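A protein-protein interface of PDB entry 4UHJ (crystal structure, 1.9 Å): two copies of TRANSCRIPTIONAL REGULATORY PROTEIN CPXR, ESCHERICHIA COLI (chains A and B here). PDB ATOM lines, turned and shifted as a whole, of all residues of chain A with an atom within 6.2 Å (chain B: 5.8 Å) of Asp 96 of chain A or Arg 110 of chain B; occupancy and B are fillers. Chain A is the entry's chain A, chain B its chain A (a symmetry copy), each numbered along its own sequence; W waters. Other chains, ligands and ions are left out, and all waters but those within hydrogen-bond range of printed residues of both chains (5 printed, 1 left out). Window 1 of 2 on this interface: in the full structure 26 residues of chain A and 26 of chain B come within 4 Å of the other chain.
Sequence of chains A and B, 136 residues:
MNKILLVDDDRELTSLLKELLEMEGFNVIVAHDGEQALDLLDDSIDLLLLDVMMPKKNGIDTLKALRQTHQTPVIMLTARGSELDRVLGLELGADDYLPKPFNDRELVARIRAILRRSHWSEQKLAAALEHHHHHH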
ATOM      1  N   VAL A  74      30.270 -23.296 -20.094  1.00  0.00           N
ATOM      2  CA  VAL A  74      31.001 -22.091 -20.484  1.00  0.00           C
ATOM      3  C   VAL A  74      30.110 -20.864 -20.257  1.00  0.00           C
ATOM      4  O   VAL A  74      28.983 -20.820 -20.740  1.00  0.00           O
ATOM      5  CB  VAL A  74      31.530 -22.127 -21.966  1.00  0.00           C
ATOM      6  CG1 VAL A  74      32.106 -20.762 -22.389  1.00  0.00           C
ATOM      7  CG2 VAL A  74      32.588 -23.227 -22.182  1.00  0.00           C
ATOM      8  N   ILE A  75      30.642 -19.864 -19.559  1.00  0.00           N
ATOM      9  CA  ILE A  75      30.009 -18.541 -19.455  1.00  0.00           C
ATOM     10  C   ILE A  75      30.926 -17.567 -20.195  1.00  0.00           C
ATOM     11  O   ILE A  75      32.097 -17.443 -19.813  1.00  0.00           O
ATOM     12  CB  ILE A  75      29.725 -18.044 -18.007  1.00  0.00           C
ATOM     13  CG1 ILE A  75      28.803 -19.002 -17.279  1.00  0.00           C
ATOM     14  CG2 ILE A  75      29.128 -16.606 -18.021  1.00  0.00           C
ATOM     15  CD1 ILE A  75      28.587 -18.674 -15.773  1.00  0.00           C
ATOM     16  N   MET A  76      30.416 -16.867 -21.230  1.00  0.00           N
ATOM     17  CA  MET A  76      31.244 -15.817 -21.853  1.00  0.00           C
ATOM     18  C   MET A  76      31.201 -14.612 -20.908  1.00  0.00           C
ATOM     19  O   MET A  76      30.136 -14.288 -20.383  1.00  0.00           O
ATOM     20  CB  MET A  76      30.748 -15.429 -23.261  1.00  0.00           C
ATOM     21  CG  MET A  76      30.585 -16.616 -24.214  1.00  0.00           C
ATOM     22  SD  MET A  76      32.077 -17.614 -24.419  1.00  0.00           S
ATOM     23  CE  MET A  76      33.115 -16.517 -25.398  1.00  0.00           C
ATOM     24  N   LEU A  77      32.341 -13.971 -20.666  1.00  0.00           N
ATOM     25  CA  LEU A  77      32.424 -12.806 -19.763  1.00  0.00           C
ATOM     26  C   LEU A  77      33.322 -11.829 -20.470  1.00  0.00           C
ATOM     27  O   LEU A  77      34.524 -12.059 -20.540  1.00  0.00           O
ATOM     28  CB  LEU A  77      32.984 -13.235 -18.388  1.00  0.00           C
ATOM     29  CG  LEU A  77      33.074 -12.096 -17.348  1.00  0.00           C
ATOM     30  CD1 LEU A  77      31.657 -11.652 -16.886  1.00  0.00           C
ATOM     31  CD2 LEU A  77      33.871 -12.542 -16.128  1.00  0.00           C
ATOM     32  N   ARG A  86      25.878 -11.480 -27.900  1.00  0.00           N
ATOM     33  CA  ARG A  86      25.336 -12.438 -26.921  1.00  0.00           C
ATOM     34  C   ARG A  86      24.765 -13.670 -27.635  1.00  0.00           C
ATOM     35  O   ARG A  86      25.113 -14.795 -27.270  1.00  0.00           O
ATOM     36  CB  ARG A  86      24.267 -11.772 -26.020  1.00  0.00           C
ATOM     37  CG  ARG A  86      24.857 -10.596 -25.252  1.00  0.00           C
ATOM     38  CD  ARG A  86      24.138 -10.259 -23.961  1.00  0.00           C
ATOM     39  NE  ARG A  86      22.760  -9.802 -24.163  1.00  0.00           N
ATOM     40  CZ  ARG A  86      22.373  -8.529 -24.214  1.00  0.00           C
ATOM     41  NH1 ARG A  86      23.266  -7.556 -24.158  1.00  0.00           N
ATOM     42  NH2 ARG A  86      21.089  -8.223 -24.339  1.00  0.00           N
ATOM     43  N   GLY A  89      27.611 -15.914 -29.159  1.00  0.00           N
ATOM     44  CA  GLY A  89      28.285 -16.707 -28.128  1.00  0.00           C
ATOM     45  C   GLY A  89      27.471 -17.923 -27.709  1.00  0.00           C
ATOM     46  O   GLY A  89      27.986 -19.043 -27.672  1.00  0.00           O
ATOM     47  N   LEU A  90      26.171 -17.730 -27.481  1.00  0.00           N
ATOM     48  CA  LEU A  90      25.262 -18.823 -27.079  1.00  0.00           C
ATOM     49  C   LEU A  90      25.143 -19.870 -28.189  1.00  0.00           C
ATOM     50  O   LEU A  90      25.275 -21.074 -27.935  1.00  0.00           O
ATOM     51  CB  LEU A  90      23.867 -18.261 -26.711  1.00  0.00           C
ATOM     52  CG  LEU A  90      23.811 -17.349 -25.481  1.00  0.00           C
ATOM     53  CD1 LEU A  90      22.496 -16.556 -25.438  1.00  0.00           C
ATOM     54  CD2 LEU A  90      23.992 -18.173 -24.173  1.00  0.00           C
ATOM     55  N   GLU A  91      24.964 -19.412 -29.424  1.00  0.00           N
ATOM     56  CA  GLU A  91      24.813 -20.289 -30.595  1.00  0.00           C
ATOM     57  C   GLU A  91      26.082 -21.074 -30.877  1.00  0.00           C
ATOM     58  O   GLU A  91      25.986 -22.194 -31.351  1.00  0.00           O
ATOM     59  CB  GLU A  91      24.403 -19.487 -31.848  1.00  0.00           C
ATOM     60  CG  GLU A  91      22.925 -19.088 -31.836  1.00  0.00           C
ATOM     61  CD  GLU A  91      21.917 -20.232 -31.854  1.00  0.00           C
ATOM     62  OE1 GLU A  91      22.139 -21.214 -32.595  1.00  0.00           O
ATOM     63  OE2 GLU A  91      20.929 -20.170 -31.086  1.00  0.00           O
ATOM     64  N   ALA A  94      28.179 -21.571 -25.892  1.00  0.00           N
ATOM     65  CA  ALA A  94      28.216 -21.099 -24.515  1.00  0.00           C
ATOM     66  C   ALA A  94      26.891 -21.331 -23.848  1.00  0.00           C
ATOM     67  O   ALA A  94      25.835 -21.253 -24.482  1.00  0.00           O
ATOM     68  CB  ALA A  94      28.574 -19.615 -24.444  1.00  0.00           C
ATOM     69  N   ASP A  95      26.952 -21.536 -22.546  1.00  0.00           N
ATOM     70  CA  ASP A  95      25.766 -21.760 -21.742  1.00  0.00           C
ATOM     71  C   ASP A  95      25.151 -20.461 -21.313  1.00  0.00           C
ATOM     72  O   ASP A  95      23.934 -20.381 -21.157  1.00  0.00           O
ATOM     73  CB  ASP A  95      26.114 -22.615 -20.528  1.00  0.00           C
ATOM     74  CG  ASP A  95      26.495 -24.024 -20.949  1.00  0.00           C
ATOM     75  OD1 ASP A  95      25.571 -24.828 -21.256  1.00  0.00           O
ATOM     76  OD2 ASP A  95      27.693 -24.273 -21.122  1.00  0.00           O
ATOM     77  N   ASP A  96      25.990 -19.463 -21.052  1.00  0.00           N
ATOM     78  CA  ASP A  96      25.547 -18.152 -20.599  1.00  0.00           C
ATOM     79  C   ASP A  96      26.523 -17.135 -21.168  1.00  0.00           C
ATOM     80  O   ASP A  96      27.546 -17.491 -21.767  1.00  0.00           O
ATOM     81  CB  ASP A  96      25.474 -18.099 -19.041  1.00  0.00           C
ATOM     82  CG  ASP A  96      24.539 -17.048 -18.430  1.00  0.00           C
ATOM     83  OD1 ASP A  96      24.174 -16.066 -19.140  1.00  0.00           O
ATOM     84  OD2 ASP A  96      24.172 -17.202 -17.254  1.00  0.00           O
ATOM     85  N   TYR A  97      26.141 -15.876 -21.065  1.00  0.00           N
ATOM     86  CA  TYR A  97      26.869 -14.758 -21.641  1.00  0.00           C
ATOM     87  C   TYR A  97      26.600 -13.575 -20.780  1.00  0.00           C
ATOM     88  O   TYR A  97      25.460 -13.143 -20.699  1.00  0.00           O
ATOM     89  CB  TYR A  97      26.372 -14.531 -23.075  1.00  0.00           C
ATOM     90  CG  TYR A  97      27.348 -13.764 -23.936  1.00  0.00           C
ATOM     91  CD1 TYR A  97      27.593 -12.409 -23.712  1.00  0.00           C
ATOM     92  CD2 TYR A  97      27.967 -14.369 -25.027  1.00  0.00           C
ATOM     93  CE1 TYR A  97      28.464 -11.683 -24.538  1.00  0.00           C
ATOM     94  CE2 TYR A  97      28.874 -13.669 -25.828  1.00  0.00           C
ATOM     95  CZ  TYR A  97      29.106 -12.322 -25.590  1.00  0.00           C
ATOM     96  OH  TYR A  97      29.952 -11.637 -26.426  1.00  0.00           O
ATOM     97  N   LEU A  98      27.637 -13.057 -20.122  1.00  0.00           N
ATOM     98  CA  LEU A  98      27.480 -11.936 -19.217  1.00  0.00           C
ATOM     99  C   LEU A  98      28.386 -10.771 -19.645  1.00  0.00           C
ATOM    100  O   LEU A  98      29.599 -10.861 -19.509  1.00  0.00           O
ATOM    101  CB  LEU A  98      27.769 -12.395 -17.776  1.00  0.00           C
ATOM    102  CG  LEU A  98      27.416 -11.381 -16.654  1.00  0.00           C
ATOM    103  CD1 LEU A  98      25.876 -11.080 -16.593  1.00  0.00           C
ATOM    104  CD2 LEU A  98      27.906 -11.893 -15.309  1.00  0.00           C
ATOM    105  N   PRO A  99      27.828  -9.670 -20.181  1.00  0.00           N
ATOM    106  CA  PRO A  99      28.700  -8.552 -20.574  1.00  0.00           C
ATOM    107  C   PRO A  99      29.399  -7.852 -19.407  1.00  0.00           C
ATOM    108  O   PRO A  99      28.846  -7.759 -18.306  1.00  0.00           O
ATOM    109  CB  PRO A  99      27.747  -7.553 -21.245  1.00  0.00           C
ATOM    110  CG  PRO A  99      26.481  -8.331 -21.536  1.00  0.00           C
ATOM    111  CD  PRO A  99      26.403  -9.387 -20.459  1.00  0.00           C
ATOM    112  N   ARG A 110      25.154 -16.781 -11.313  1.00  0.00           N
ATOM    113  CA  ARG A 110      25.113 -17.477 -12.612  1.00  0.00           C
ATOM    114  C   ARG A 110      26.073 -18.671 -12.610  1.00  0.00           C
ATOM    115  O   ARG A 110      25.730 -19.728 -13.135  1.00  0.00           O
ATOM    116  CB  ARG A 110      25.395 -16.515 -13.783  1.00  0.00           C
ATOM    117  CG  ARG A 110      24.202 -15.554 -13.995  1.00  0.00           C
ATOM    118  CD  ARG A 110      24.349 -14.571 -15.129  1.00  0.00           C
ATOM    119  NE  ARG A 110      23.123 -13.779 -15.278  1.00  0.00           N
ATOM    120  CZ  ARG A 110      22.024 -14.184 -15.907  1.00  0.00           C
ATOM    121  NH1 ARG A 110      21.991 -15.375 -16.507  1.00  0.00           N
ATOM    122  NH2 ARG A 110      20.946 -13.413 -15.932  1.00  0.00           N
ATOM    123  N   ILE A 114      24.586 -22.625 -12.913  1.00  0.00           N
ATOM    124  CA  ILE A 114      25.048 -23.624 -13.884  1.00  0.00           C
ATOM    125  C   ILE A 114      25.660 -24.842 -13.183  1.00  0.00           C
ATOM    126  O   ILE A 114      25.383 -25.971 -13.603  1.00  0.00           O
ATOM    127  CB  ILE A 114      25.999 -23.025 -14.936  1.00  0.00           C
ATOM    128  CG1 ILE A 114      25.251 -21.976 -15.737  1.00  0.00           C
ATOM    129  CG2 ILE A 114      26.513 -24.112 -15.852  1.00  0.00           C
ATOM    130  CD1 ILE A 114      26.047 -21.149 -16.663  1.00  0.00           C
ATOM    131  N   ILE B  75      13.688 -20.590 -17.005  1.00  0.00           N
ATOM    132  CA  ILE B  75      14.172 -19.243 -17.342  1.00  0.00           C
ATOM    133  C   ILE B  75      13.145 -18.263 -16.773  1.00  0.00           C
ATOM    134  O   ILE B  75      11.971 -18.337 -17.159  1.00  0.00           O
ATOM    135  CB  ILE B  75      14.414 -18.975 -18.856  1.00  0.00           C
ATOM    136  CG1 ILE B  75      15.442 -19.937 -19.417  1.00  0.00           C
ATOM    137  CG2 ILE B  75      14.847 -17.499 -19.098  1.00  0.00           C
ATOM    138  CD1 ILE B  75      15.636 -19.852 -20.959  1.00  0.00           C
ATOM    139  N   ASP B  95      17.512 -21.301 -13.809  1.00  0.00           N
ATOM    140  CA  ASP B  95      18.723 -21.528 -14.573  1.00  0.00           C
ATOM    141  C   ASP B  95      19.195 -20.263 -15.227  1.00  0.00           C
ATOM    142  O   ASP B  95      20.396 -20.076 -15.406  1.00  0.00           O
ATOM    143  CB  ASP B  95      18.483 -22.613 -15.619  1.00  0.00           C
ATOM    144  CG  ASP B  95      18.257 -23.961 -14.957  1.00  0.00           C
ATOM    145  OD1 ASP B  95      19.261 -24.593 -14.524  1.00  0.00           O
ATOM    146  OD2 ASP B  95      17.092 -24.308 -14.732  1.00  0.00           O
ATOM    147  N   ASP B  96      18.253 -19.424 -15.649  1.00  0.00           N
ATOM    148  CA  ASP B  96      18.552 -18.170 -16.325  1.00  0.00           C
ATOM    149  C   ASP B  96      17.464 -17.185 -15.932  1.00  0.00           C
ATOM    150  O   ASP B  96      16.481 -17.543 -15.271  1.00  0.00           O
ATOM    151  CB  ASP B  96      18.634 -18.379 -17.870  1.00  0.00           C
ATOM    152  CG  ASP B  96      19.452 -17.353 -18.663  1.00  0.00           C
ATOM    153  OD1 ASP B  96      19.700 -16.229 -18.137  1.00  0.00           O
ATOM    154  OD2 ASP B  96      19.846 -17.667 -19.798  1.00  0.00           O
ATOM    155  N   LEU B  98      15.915 -13.497 -17.656  1.00  0.00           N
ATOM    156  CA  LEU B  98      15.955 -12.539 -18.742  1.00  0.00           C
ATOM    157  C   LEU B  98      14.922 -11.426 -18.514  1.00  0.00           C
ATOM    158  O   LEU B  98      13.728 -11.672 -18.621  1.00  0.00           O
ATOM    159  CB  LEU B  98      15.733 -13.270 -20.080  1.00  0.00           C
ATOM    160  CG  LEU B  98      15.983 -12.433 -21.363  1.00  0.00           C
ATOM    161  CD1 LEU B  98      17.480 -11.978 -21.490  1.00  0.00           C
ATOM    162  CD2 LEU B  98      15.565 -13.220 -22.595  1.00  0.00           C
ATOM    163  N   ARG B 105      15.499 -12.683 -30.313  1.00  0.00           N
ATOM    164  CA  ARG B 105      16.597 -13.555 -30.724  1.00  0.00           C
ATOM    165  C   ARG B 105      17.414 -14.034 -29.538  1.00  0.00           C
ATOM    166  O   ARG B 105      17.835 -15.186 -29.537  1.00  0.00           O
ATOM    167  CB  ARG B 105      17.500 -12.885 -31.773  1.00  0.00           C
ATOM    168  CG  ARG B 105      16.799 -12.470 -33.108  1.00  0.00           C
ATOM    169  CD  ARG B 105      15.723 -13.429 -33.631  1.00  0.00           C
ATOM    170  NE  ARG B 105      16.208 -14.808 -33.773  1.00  0.00           N
ATOM    171  CZ  ARG B 105      15.427 -15.886 -33.759  1.00  0.00           C
ATOM    172  NH1 ARG B 105      14.110 -15.760 -33.650  1.00  0.00           N
ATOM    173  NH2 ARG B 105      15.954 -17.094 -33.880  1.00  0.00           N
ATOM    174  N   GLU B 106      17.632 -13.178 -28.544  1.00  0.00           N
ATOM    175  CA  GLU B 106      18.389 -13.586 -27.357  1.00  0.00           C
ATOM    176  C   GLU B 106      17.593 -14.620 -26.554  1.00  0.00           C
ATOM    177  O   GLU B 106      18.176 -15.596 -26.063  1.00  0.00           O
ATOM    178  CB  GLU B 106      18.746 -12.375 -26.489  1.00  0.00           C
ATOM    179  CG  GLU B 106      19.619 -12.782 -25.311  1.00  0.00           C
ATOM    180  CD  GLU B 106      20.053 -11.689 -24.366  1.00  0.00           C
ATOM    181  OE1 GLU B 106      19.634 -10.520 -24.530  1.00  0.00           O
ATOM    182  OE2 GLU B 106      20.871 -12.009 -23.480  1.00  0.00           O
ATOM    183  N   LEU B 107      16.269 -14.400 -26.415  1.00  0.00           N
ATOM    184  CA  LEU B 107      15.413 -15.359 -25.720  1.00  0.00           C
ATOM    185  C   LEU B 107      15.515 -16.741 -26.399  1.00  0.00           C
ATOM    186  O   LEU B 107      15.726 -17.730 -25.703  1.00  0.00           O
ATOM    187  CB  LEU B 107      13.936 -14.878 -25.679  1.00  0.00           C
ATOM    188  CG  LEU B 107      12.903 -15.917 -25.154  1.00  0.00           C
ATOM    189  CD1 LEU B 107      13.198 -16.346 -23.724  1.00  0.00           C
ATOM    190  CD2 LEU B 107      11.501 -15.359 -25.218  1.00  0.00           C
ATOM    191  N   VAL B 108      15.350 -16.799 -27.724  1.00  0.00           N
ATOM    192  CA  VAL B 108      15.424 -18.058 -28.499  1.00  0.00           C
ATOM    193  C   VAL B 108      16.821 -18.712 -28.307  1.00  0.00           C
ATOM    194  O   VAL B 108      16.893 -19.927 -28.073  1.00  0.00           O
ATOM    195  CB  VAL B 108      15.026 -17.900 -30.004  1.00  0.00           C
ATOM    196  CG1 VAL B 108      15.265 -19.195 -30.789  1.00  0.00           C
ATOM    197  CG2 VAL B 108      13.554 -17.522 -30.130  1.00  0.00           C
ATOM    198  N   ALA B 109      17.897 -17.917 -28.346  1.00  0.00           N
ATOM    199  CA  ALA B 109      19.246 -18.467 -28.173  1.00  0.00           C
ATOM    200  C   ALA B 109      19.436 -19.039 -26.750  1.00  0.00           C
ATOM    201  O   ALA B 109      20.090 -20.072 -26.619  1.00  0.00           O
ATOM    202  CB  ALA B 109      20.319 -17.412 -28.483  1.00  0.00           C
ATOM    203  N   ARG B 110      18.881 -18.390 -25.712  1.00  0.00           N
ATOM    204  CA  ARG B 110      18.986 -18.842 -24.313  1.00  0.00           C
ATOM    205  C   ARG B 110      18.164 -20.117 -24.100  1.00  0.00           C
ATOM    206  O   ARG B 110      18.617 -21.023 -23.402  1.00  0.00           O
ATOM    207  CB  ARG B 110      18.587 -17.730 -23.323  1.00  0.00           C
ATOM    208  CG  ARG B 110      19.665 -16.620 -23.292  1.00  0.00           C
ATOM    209  CD  ARG B 110      19.399 -15.478 -22.343  1.00  0.00           C
ATOM    210  NE  ARG B 110      20.528 -14.542 -22.346  1.00  0.00           N
ATOM    211  CZ  ARG B 110      21.659 -14.707 -21.667  1.00  0.00           C
ATOM    212  NH1 ARG B 110      21.818 -15.766 -20.870  1.00  0.00           N
ATOM    213  NH2 ARG B 110      22.644 -13.829 -21.786  1.00  0.00           N
ATOM    214  N   ILE B 111      16.983 -20.214 -24.744  1.00  0.00           N
ATOM    215  CA  ILE B 111      16.174 -21.439 -24.718  1.00  0.00           C
ATOM    216  C   ILE B 111      16.994 -22.578 -25.347  1.00  0.00           C
ATOM    217  O   ILE B 111      17.123 -23.663 -24.757  1.00  0.00           O
ATOM    218  CB  ILE B 111      14.808 -21.240 -25.444  1.00  0.00           C
ATOM    219  CG1 ILE B 111      13.904 -20.326 -24.616  1.00  0.00           C
ATOM    220  CG2 ILE B 111      14.129 -22.615 -25.743  1.00  0.00           C
ATOM    221  CD1 ILE B 111      12.614 -19.827 -25.312  1.00  0.00           C
ATOM    222  N   ARG B 112      17.558 -22.310 -26.521  1.00  0.00           N
ATOM    223  CA  ARG B 112      18.340 -23.303 -27.267  1.00  0.00           C
ATOM    224  C   ARG B 112      19.587 -23.726 -26.487  1.00  0.00           C
ATOM    225  O   ARG B 112      19.892 -24.910 -26.455  1.00  0.00           O
ATOM    226  CB  ARG B 112      18.700 -22.771 -28.658  1.00  0.00           C
ATOM    227  CG  ARG B 112      17.499 -22.876 -29.630  1.00  0.00           C
ATOM    228  CD  ARG B 112      17.659 -22.055 -30.907  1.00  0.00           C
ATOM    229  NE  ARG B 112      18.924 -22.287 -31.612  1.00  0.00           N
ATOM    230  CZ  ARG B 112      19.054 -23.185 -32.572  1.00  0.00           C
ATOM    231  NH1 ARG B 112      18.018 -23.940 -32.922  1.00  0.00           N
ATOM    232  NH2 ARG B 112      20.214 -23.343 -33.189  1.00  0.00           N
ATOM    233  N   ALA B 113      20.269 -22.784 -25.808  1.00  0.00           N
ATOM    234  CA  ALA B 113      21.488 -23.094 -25.031  1.00  0.00           C
ATOM    235  C   ALA B 113      21.168 -24.041 -23.852  1.00  0.00           C
ATOM    236  O   ALA B 113      21.869 -25.033 -23.632  1.00  0.00           O
ATOM    237  CB  ALA B 113      22.137 -21.799 -24.524  1.00  0.00           C
ATOM    238  N   ILE B 114      20.077 -23.770 -23.132  1.00  0.00           N
ATOM    239  CA  ILE B 114      19.719 -24.631 -21.998  1.00  0.00           C
ATOM    240  C   ILE B 114      19.253 -26.013 -22.472  1.00  0.00           C
ATOM    241  O   ILE B 114      19.649 -27.014 -21.865  1.00  0.00           O
ATOM    242  CB  ILE B 114      18.697 -23.969 -21.056  1.00  0.00           C
ATOM    243  CG1 ILE B 114      19.317 -22.720 -20.455  1.00  0.00           C
ATOM    244  CG2 ILE B 114      18.298 -24.931 -19.961  1.00  0.00           C
ATOM    245  CD1 ILE B 114      18.425 -21.839 -19.679  1.00  0.00           C
ATOM    246  N   LEU B 115      18.481 -26.071 -23.566  1.00  0.00           N
ATOM    247  CA  LEU B 115      17.989 -27.357 -24.090  1.00  0.00           C
ATOM    248  C   LEU B 115      19.109 -28.171 -24.726  1.00  0.00           C
ATOM    249  O   LEU B 115      19.061 -29.402 -24.699  1.00  0.00           O
ATOM    250  CB  LEU B 115      16.835 -27.153 -25.068  1.00  0.00           C
ATOM    251  CG  LEU B 115      15.539 -26.590 -24.430  1.00  0.00           C
ATOM    252  CD1 LEU B 115      14.493 -26.336 -25.476  1.00  0.00           C
ATOM    253  CD2 LEU B 115      14.963 -27.535 -23.353  1.00  0.00           C
HETATM  254  O   HOH W   1      21.168 -10.482 -21.286  1.00  0.00           O
HETATM  255  O   HOH W   2      24.538 -24.949 -23.787  1.00  0.00           O
HETATM  256  O   HOH W   3      19.768 -13.708 -19.152  1.00  0.00           O
HETATM  257  O   HOH W   4      18.677 -19.085 -32.085  1.00  0.00           O
HETATM  258  O   HOH W   5      23.817 -13.431 -18.575  1.00  0.00           O
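The side-chain carboxylate of Asp 96 of chain A is in salt-bridge range of the guanidinium group of Arg 110 of chain B, 2.9 Å away.
NH2 of Arg 110 of chain B lies within hydrogen-bond range of O of Tyr 97 of chain A (3.1 Å).
The side-chain carboxylate (OD1) of Asp 96 of chain B lies within salt-bridge range of the guanidinium group (NH1) of Arg 110 of chain A (2.9 Å).
NH2 of Arg 86 of chain A lies within salt-bridge range of OE1 of Glu 106 of chain B (2.7 Å).
The side-chain carboxylate (OE1) of Glu 91 of chain A is in salt-bridge range of the guanidinium group (NH2) of Arg 112 of chain B (2.9 Å).
The backbone carbonyl oxygen of Val 74 of chain A is in hydrogen-bond range of the backbone NH of Asp 96 of chain A (3.3 Å).
The guanidinium group (NH1) of Arg 110 of chain B is in salt-bridge range of the side-chain carboxylate (OD2) of Asp 96 of chain B (2.9 Å).
N of Ala 94 of chain A sits at hydrogen-bond distance from O of Gly 89 of chain A (3.1 Å).
OD2 of Asp 96 of chain A lies within salt-bridge range of NH1 of Arg 110 of chain A (2.9 Å).
N of Met 76 of chain A sits at hydrogen-bond distance from O of Asp 96 of chain A (3.0 Å).
The side-chain carboxylate (OE2) of Glu 106 of chain B is in salt-bridge range of the guanidinium group (NE) of Arg 110 of chain B, 2.8 Å away.
Among the printed residues, pairs that only touch across the chains: Leu 90 of chain A with Ala 109 of chain B, Leu 90 of chain A with Arg 110 of chain B, Glu 91 of chain A with Ala 109 of chain B and Ala 94 of chain A with Ala 113 of chain B.
Asp 96 of chain A touches one residue of chain B.
Printed residues of chain B within 4 Å of Tyr 97 of chain A: Arg 110 (3.1 Å).
Arg 110 of chain B touches three residues of chain A.
Of the printed residues of chain A, Arg 112 of chain B touches Glu 91.
Of the printed residues of chain A, Ala 113 of chain B touches Ala 94.
Leu 115 of chain B touches none of the printed residues of chain A.
Of the 15 printed residues of chain B, 6 touch a printed residue of chain A.
Of the 16 printed residues of chain A, 7 touch a printed residue of chain B.
Printed residues of chain A that touch a printed residue of chain B: Arg 86, Leu 90, Glu 91, Ala 94, Asp 96, Tyr 97 and Arg 110.
Hydrophobic or aromatic side chains of chain A within 4 Å of the printed part of chain B: Leu 90.
Among the printed residues, 9 pairs touch across the chains.
Among the printed residues, Asp or Glu carboxylates within 4 Å of a Lys or Arg side-chain nitrogen of the other chain: Arg 86 of chain A with Glu 106 of chain B (2.7 Å), Glu 91 of chain A with Arg 112 of chain B (2.9 Å), Asp 96 of chain A with Arg 110 of chain B (2.9 Å) and Arg 110 of chain A with Asp 96 of chain B (2.9 Å).
Asp 96 of chain A touches Arg 110 of chain B, and with the chains exchanged Arg 110 of chain A touches Asp 96 of chain B.
Positions printed for both chains: 75, 95, 96, 98, 110 and 114.
Of the 9 pairs that touch across the chains among the printed residues, 2 have their exchanged pair printed and touching as well.
Water W2 bridges the backbone carbonyl oxygen of Ala 113 of chain B (2.7 Å) and the side-chain carboxylate of Asp 95 of chain A (2.7 Å).
Water W1 bridges OE2 of Glu 106 of chain B and NE of Arg 86 of chain A.
Water W4 lies within hydrogen-bond range of OE2 of Glu 91 of chain A (2.7 Å) and NE of Arg 112 of chain B (3.2 Å).
Water W5 lies within hydrogen-bond range of O of Tyr 97 of chain A, OD1 of Asp 96 of chain A, NH1 of Arg 110 of chain A and NH2 of Arg 110 of chain B.
Water W3 lies within hydrogen-bond range of OD1 of Asp 96 of chain B (2.7 Å), NH1 of Arg 110 of chain B (3.4 Å) and NH2 of Arg 110 of chain A (3.4 Å).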
